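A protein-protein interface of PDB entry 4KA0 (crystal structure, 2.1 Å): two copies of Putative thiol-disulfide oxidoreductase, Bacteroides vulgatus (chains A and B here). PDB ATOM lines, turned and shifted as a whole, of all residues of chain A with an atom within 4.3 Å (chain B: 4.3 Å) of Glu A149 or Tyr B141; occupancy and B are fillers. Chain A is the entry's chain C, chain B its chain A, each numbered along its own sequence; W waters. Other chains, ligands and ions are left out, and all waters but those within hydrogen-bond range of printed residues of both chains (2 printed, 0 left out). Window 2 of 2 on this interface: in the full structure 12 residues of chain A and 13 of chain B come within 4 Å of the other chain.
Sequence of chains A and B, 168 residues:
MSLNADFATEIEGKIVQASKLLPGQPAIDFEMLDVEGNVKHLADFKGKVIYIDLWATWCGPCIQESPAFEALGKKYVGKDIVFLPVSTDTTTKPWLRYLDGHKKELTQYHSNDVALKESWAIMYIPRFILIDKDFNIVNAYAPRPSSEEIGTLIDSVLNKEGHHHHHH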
ATOM      1  N   ASN A 139       6.822 -30.148  -5.341  1.00  0.00           N
ATOM      2  CA  ASN A 139       7.858 -29.123  -5.462  1.00  0.00           C
ATOM      3  C   ASN A 139       8.912 -29.403  -4.386  1.00  0.00           C
ATOM      4  O   ASN A 139       8.685 -29.190  -3.211  1.00  0.00           O
ATOM      5  CB  ASN A 139       7.236 -27.699  -5.300  1.00  0.00           C
ATOM      6  CG  ASN A 139       8.256 -26.521  -5.456  1.00  0.00           C
ATOM      7  OD1 ASN A 139       9.460 -26.639  -5.176  1.00  0.00           O
ATOM      8  ND2 ASN A 139       7.733 -25.346  -5.822  1.00  0.00           N
ATOM      9  N   PRO A 143       7.344 -23.193  -1.830  1.00  0.00           N
ATOM     10  CA  PRO A 143       7.249 -21.898  -1.139  1.00  0.00           C
ATOM     11  C   PRO A 143       7.259 -22.060   0.369  1.00  0.00           C
ATOM     12  O   PRO A 143       6.936 -23.156   0.889  1.00  0.00           O
ATOM     13  CB  PRO A 143       5.854 -21.401  -1.518  1.00  0.00           C
ATOM     14  CG  PRO A 143       5.508 -22.130  -2.775  1.00  0.00           C
ATOM     15  CD  PRO A 143       6.248 -23.414  -2.781  1.00  0.00           C
ATOM     16  N   SER A 147       4.056 -17.612   3.059  1.00  0.00           N
ATOM     17  CA  SER A 147       3.659 -17.040   1.773  1.00  0.00           C
ATOM     18  C   SER A 147       2.180 -17.266   1.525  1.00  0.00           C
ATOM     19  O   SER A 147       1.603 -18.242   2.013  1.00  0.00           O
ATOM     20  CB  SER A 147       4.439 -17.662   0.628  1.00  0.00           C
ATOM     21  OG  SER A 147       4.078 -19.028   0.411  1.00  0.00           O
ATOM     22  N   GLU A 148       1.575 -16.361   0.757  1.00  0.00           N
ATOM     23  CA  GLU A 148       0.199 -16.540   0.262  1.00  0.00           C
ATOM     24  C   GLU A 148       0.159 -17.712  -0.689  1.00  0.00           C
ATOM     25  O   GLU A 148      -0.801 -18.431  -0.744  1.00  0.00           O
ATOM     26  CB  GLU A 148      -0.261 -15.301  -0.509  1.00  0.00           C
ATOM     27  CG  GLU A 148       0.093 -13.994   0.159  1.00  0.00           C
ATOM     28  CD  GLU A 148      -0.314 -14.015   1.620  1.00  0.00           C
ATOM     29  OE1 GLU A 148      -1.484 -14.405   1.893  1.00  0.00           O
ATOM     30  OE2 GLU A 148       0.537 -13.677   2.481  1.00  0.00           O
ATOM     31  N   GLU A 149       1.228 -17.890  -1.450  1.00  0.00           N
ATOM     32  CA  GLU A 149       1.329 -18.935  -2.475  1.00  0.00           C
ATOM     33  C   GLU A 149       1.210 -20.413  -1.938  1.00  0.00           C
ATOM     34  O   GLU A 149       0.728 -21.314  -2.654  1.00  0.00           O
ATOM     35  CB  GLU A 149       2.663 -18.730  -3.216  1.00  0.00           C
ATOM     36  CG  GLU A 149       2.667 -17.494  -4.119  1.00  0.00           C
ATOM     37  CD  GLU A 149       3.023 -16.165  -3.452  1.00  0.00           C
ATOM     38  OE1 GLU A 149       3.497 -16.130  -2.310  1.00  0.00           O
ATOM     39  OE2 GLU A 149       2.867 -15.100  -4.100  1.00  0.00           O
ATOM     40  N   ILE A 150       1.634 -20.667  -0.690  1.00  0.00           N
ATOM     41  CA  ILE A 150       1.602 -22.079  -0.165  1.00  0.00           C
ATOM     42  C   ILE A 150       0.191 -22.609   0.048  1.00  0.00           C
ATOM     43  O   ILE A 150      -0.125 -23.718  -0.331  1.00  0.00           O
ATOM     44  CB  ILE A 150       2.446 -22.299   1.133  1.00  0.00           C
ATOM     45  CG1 ILE A 150       2.527 -23.804   1.455  1.00  0.00           C
ATOM     46  CG2 ILE A 150       1.840 -21.544   2.331  1.00  0.00           C
ATOM     47  CD1 ILE A 150       3.274 -24.662   0.414  1.00  0.00           C
ATOM     48  N   GLY A 151      -0.693 -21.813   0.615  1.00  0.00           N
ATOM     49  CA  GLY A 151      -2.087 -22.252   0.728  1.00  0.00           C
ATOM     50  C   GLY A 151      -2.784 -22.685  -0.551  1.00  0.00           C
ATOM     51  O   GLY A 151      -3.564 -23.656  -0.570  1.00  0.00           O
ATOM     52  N   THR A 152      -2.542 -21.942  -1.627  1.00  0.00           N
ATOM     53  CA  THR A 152      -3.232 -22.208  -2.898  1.00  0.00           C
ATOM     54  C   THR A 152      -2.600 -23.475  -3.413  1.00  0.00           C
ATOM     55  O   THR A 152      -3.292 -24.360  -3.886  1.00  0.00           O
ATOM     56  CB  THR A 152      -3.014 -21.069  -3.919  1.00  0.00           C
ATOM     57  OG1 THR A 152      -3.157 -19.813  -3.262  1.00  0.00           O
ATOM     58  CG2 THR A 152      -4.006 -21.144  -5.028  1.00  0.00           C
ATOM     59  N   LEU A 153      -1.276 -23.571  -3.248  1.00  0.00           N
ATOM     60  CA  LEU A 153      -0.542 -24.762  -3.679  1.00  0.00           C
ATOM     61  C   LEU A 153      -1.129 -25.991  -2.997  1.00  0.00           C
ATOM     62  O   LEU A 153      -1.508 -26.960  -3.659  1.00  0.00           O
ATOM     63  CB  LEU A 153       0.960 -24.646  -3.411  1.00  0.00           C
ATOM     64  CG  LEU A 153       1.864 -25.725  -4.011  1.00  0.00           C
ATOM     65  CD1 LEU A 153       1.514 -26.039  -5.450  1.00  0.00           C
ATOM     66  CD2 LEU A 153       3.345 -25.381  -3.939  1.00  0.00           C
ATOM     67  N   TYR B 124       0.146 -11.864  -6.451  1.00  0.00           N
ATOM     68  CA  TYR B 124       1.211 -11.239  -5.702  1.00  0.00           C
ATOM     69  C   TYR B 124       2.536 -11.394  -6.452  1.00  0.00           C
ATOM     70  O   TYR B 124       2.777 -12.411  -7.097  1.00  0.00           O
ATOM     71  CB  TYR B 124       1.352 -11.896  -4.329  1.00  0.00           C
ATOM     72  CG  TYR B 124       0.074 -12.033  -3.513  1.00  0.00           C
ATOM     73  CD1 TYR B 124      -0.431 -10.955  -2.773  1.00  0.00           C
ATOM     74  CD2 TYR B 124      -0.617 -13.247  -3.457  1.00  0.00           C
ATOM     75  CE1 TYR B 124      -1.612 -11.092  -2.024  1.00  0.00           C
ATOM     76  CE2 TYR B 124      -1.813 -13.387  -2.715  1.00  0.00           C
ATOM     77  CZ  TYR B 124      -2.284 -12.306  -2.004  1.00  0.00           C
ATOM     78  OH  TYR B 124      -3.422 -12.430  -1.269  1.00  0.00           O
ATOM     79  N   ARG B 127       7.156 -13.053  -8.233  1.00  0.00           N
ATOM     80  CA  ARG B 127       6.687 -14.338  -8.589  1.00  0.00           C
ATOM     81  C   ARG B 127       7.591 -14.842  -9.719  1.00  0.00           C
ATOM     82  O   ARG B 127       7.917 -14.073 -10.615  1.00  0.00           O
ATOM     83  CB  ARG B 127       5.221 -14.235  -9.058  1.00  0.00           C
ATOM     84  CG  ARG B 127       4.579 -15.506  -9.572  1.00  0.00           C
ATOM     85  CD  ARG B 127       4.563 -16.649  -8.589  1.00  0.00           C
ATOM     86  NE  ARG B 127       3.802 -17.764  -9.129  1.00  0.00           N
ATOM     87  CZ  ARG B 127       2.467 -17.804  -9.146  1.00  0.00           C
ATOM     88  NH1 ARG B 127       1.748 -16.801  -8.636  1.00  0.00           N
ATOM     89  NH2 ARG B 127       1.850 -18.841  -9.689  1.00  0.00           N
ATOM     90  N   PHE B 128       7.956 -16.130  -9.645  1.00  0.00           N
ATOM     91  CA  PHE B 128       8.812 -16.765 -10.592  1.00  0.00           C
ATOM     92  C   PHE B 128       8.159 -18.060 -11.014  1.00  0.00           C
ATOM     93  O   PHE B 128       7.609 -18.818 -10.222  1.00  0.00           O
ATOM     94  CB  PHE B 128      10.192 -17.021  -9.959  1.00  0.00           C
ATOM     95  CG  PHE B 128      10.772 -15.798  -9.368  1.00  0.00           C
ATOM     96  CD1 PHE B 128      11.478 -14.934 -10.146  1.00  0.00           C
ATOM     97  CD2 PHE B 128      10.576 -15.498  -8.067  1.00  0.00           C
ATOM     98  CE1 PHE B 128      11.958 -13.744  -9.629  1.00  0.00           C
ATOM     99  CE2 PHE B 128      11.060 -14.329  -7.524  1.00  0.00           C
ATOM    100  CZ  PHE B 128      11.733 -13.440  -8.319  1.00  0.00           C
ATOM    101  N   ASN B 139       7.473 -25.697 -12.216  1.00  0.00           N
ATOM    102  CA  ASN B 139       7.015 -25.108 -10.968  1.00  0.00           C
ATOM    103  C   ASN B 139       6.378 -23.741 -11.181  1.00  0.00           C
ATOM    104  O   ASN B 139       7.015 -22.800 -11.695  1.00  0.00           O
ATOM    105  CB  ASN B 139       8.153 -24.975  -9.983  1.00  0.00           C
ATOM    106  CG  ASN B 139       8.576 -26.330  -9.455  1.00  0.00           C
ATOM    107  OD1 ASN B 139       9.667 -26.782  -9.761  1.00  0.00           O
ATOM    108  ND2 ASN B 139       7.645 -27.044  -8.744  1.00  0.00           N
ATOM    109  N   ALA B 140       5.107 -23.662 -10.794  1.00  0.00           N
ATOM    110  CA  ALA B 140       4.306 -22.430 -10.951  1.00  0.00           C
ATOM    111  C   ALA B 140       4.771 -21.469  -9.927  1.00  0.00           C
ATOM    112  O   ALA B 140       4.568 -20.251 -10.045  1.00  0.00           O
ATOM    113  CB  ALA B 140       2.808 -22.727 -10.794  1.00  0.00           C
ATOM    114  N   TYR B 141       5.405 -22.023  -8.895  1.00  0.00           N
ATOM    115  CA  TYR B 141       5.958 -21.234  -7.816  1.00  0.00           C
ATOM    116  C   TYR B 141       7.433 -21.574  -7.670  1.00  0.00           C
ATOM    117  O   TYR B 141       7.834 -22.290  -6.769  1.00  0.00           O
ATOM    118  CB  TYR B 141       5.206 -21.572  -6.522  1.00  0.00           C
ATOM    119  CG  TYR B 141       3.717 -21.308  -6.612  1.00  0.00           C
ATOM    120  CD1 TYR B 141       3.206 -20.018  -6.425  1.00  0.00           C
ATOM    121  CD2 TYR B 141       2.836 -22.346  -6.896  1.00  0.00           C
ATOM    122  CE1 TYR B 141       1.847 -19.780  -6.501  1.00  0.00           C
ATOM    123  CE2 TYR B 141       1.474 -22.126  -6.971  1.00  0.00           C
ATOM    124  CZ  TYR B 141       0.989 -20.830  -6.781  1.00  0.00           C
ATOM    125  OH  TYR B 141      -0.348 -20.625  -6.868  1.00  0.00           O
ATOM    126  N   ALA B 142       8.241 -21.069  -8.593  1.00  0.00           N
ATOM    127  CA  ALA B 142       9.637 -21.462  -8.701  1.00  0.00           C
ATOM    128  C   ALA B 142      10.455 -20.733  -7.643  1.00  0.00           C
ATOM    129  O   ALA B 142      10.054 -19.746  -7.112  1.00  0.00           O
ATOM    130  CB  ALA B 142      10.137 -21.127 -10.084  1.00  0.00           C
ATOM    131  N   PRO B 143      11.635 -21.230  -7.325  1.00  0.00           N
ATOM    132  CA  PRO B 143      12.544 -20.514  -6.433  1.00  0.00           C
ATOM    133  C   PRO B 143      13.024 -19.136  -6.964  1.00  0.00           C
ATOM    134  O   PRO B 143      13.001 -18.939  -8.138  1.00  0.00           O
ATOM    135  CB  PRO B 143      13.746 -21.470  -6.326  1.00  0.00           C
ATOM    136  CG  PRO B 143      13.241 -22.799  -6.758  1.00  0.00           C
ATOM    137  CD  PRO B 143      12.107 -22.575  -7.688  1.00  0.00           C
HETATM  138  O   HOH W   1       2.272 -15.073  -6.519  1.00  0.00           O
HETATM  139  O   HOH W   2      10.337 -27.959  -7.686  1.00  0.00           O
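Glu A149 touches just these residues of chain B: Tyr B124 (3.6 Å) and Tyr B141 (3.4 Å).
Of the printed residues of chain A, Tyr B141 touches Asn A139 (3.2 Å), Pro A143 (3.8 Å) and Glu A149 (3.4 Å).
Of the printed residues of chain A, Asn B139 touches Asn A139.
Printed residues of chain B within 4 Å of Asn A139: Asn B139 and Tyr B141.
Of the printed residues of chain B, Pro A143 touches Tyr B141 (3.8 Å).
Printed residues of chain A within 4 Å of Tyr B124: Glu A148 and Glu A149.
Phe B128 touches none of the printed residues of chain A.
Hydrophobic or aromatic side chains of chain A that line the printed part of chain B: Pro A143.
Hydrophobic or aromatic side chains of chain B that line the printed part of chain A: Tyr B124 and Tyr B141.
Among the printed residues, 6 pairs touch across the chains.
Among the printed residues, no Asp or Glu carboxylate lies within 4 Å of a Lys or Arg side-chain nitrogen of the other chain.
Among the printed residues, merely in contact across the chains: Glu A148 with Tyr B124, Glu A149 with Tyr B141, Glu A149 with Tyr B124 and Pro A143 with Tyr B141.
Asn A139 touches its own counterpart, Asn B139.
Positions printed for both chains: 139 and 143.
Of the 6 pairs that touch across the chains among the printed residues, 1 has its exchanged pair printed and touching as well.
Water W2 lies within hydrogen-bond range of OD1 of Asn B139 (2.5 Å) and OD1 of Asn A139 (3.0 Å).
Water W1 lies within hydrogen-bond range of the side-chain carboxylate (OE2) of Glu A149 (2.5 Å), the backbone carbonyl oxygen (O) of Tyr B124 (2.8 Å) and the guanidinium group (NH1) of Arg B127 (2.8 Å).
ND2 of Asn A139 lies close to ND2 of Asn B139 (3.4 Å).
The side-chain amide nitrogen of Asn A139 is in hydrogen-bond range of the backbone carbonyl oxygen of Tyr B141 (3.2 Å).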
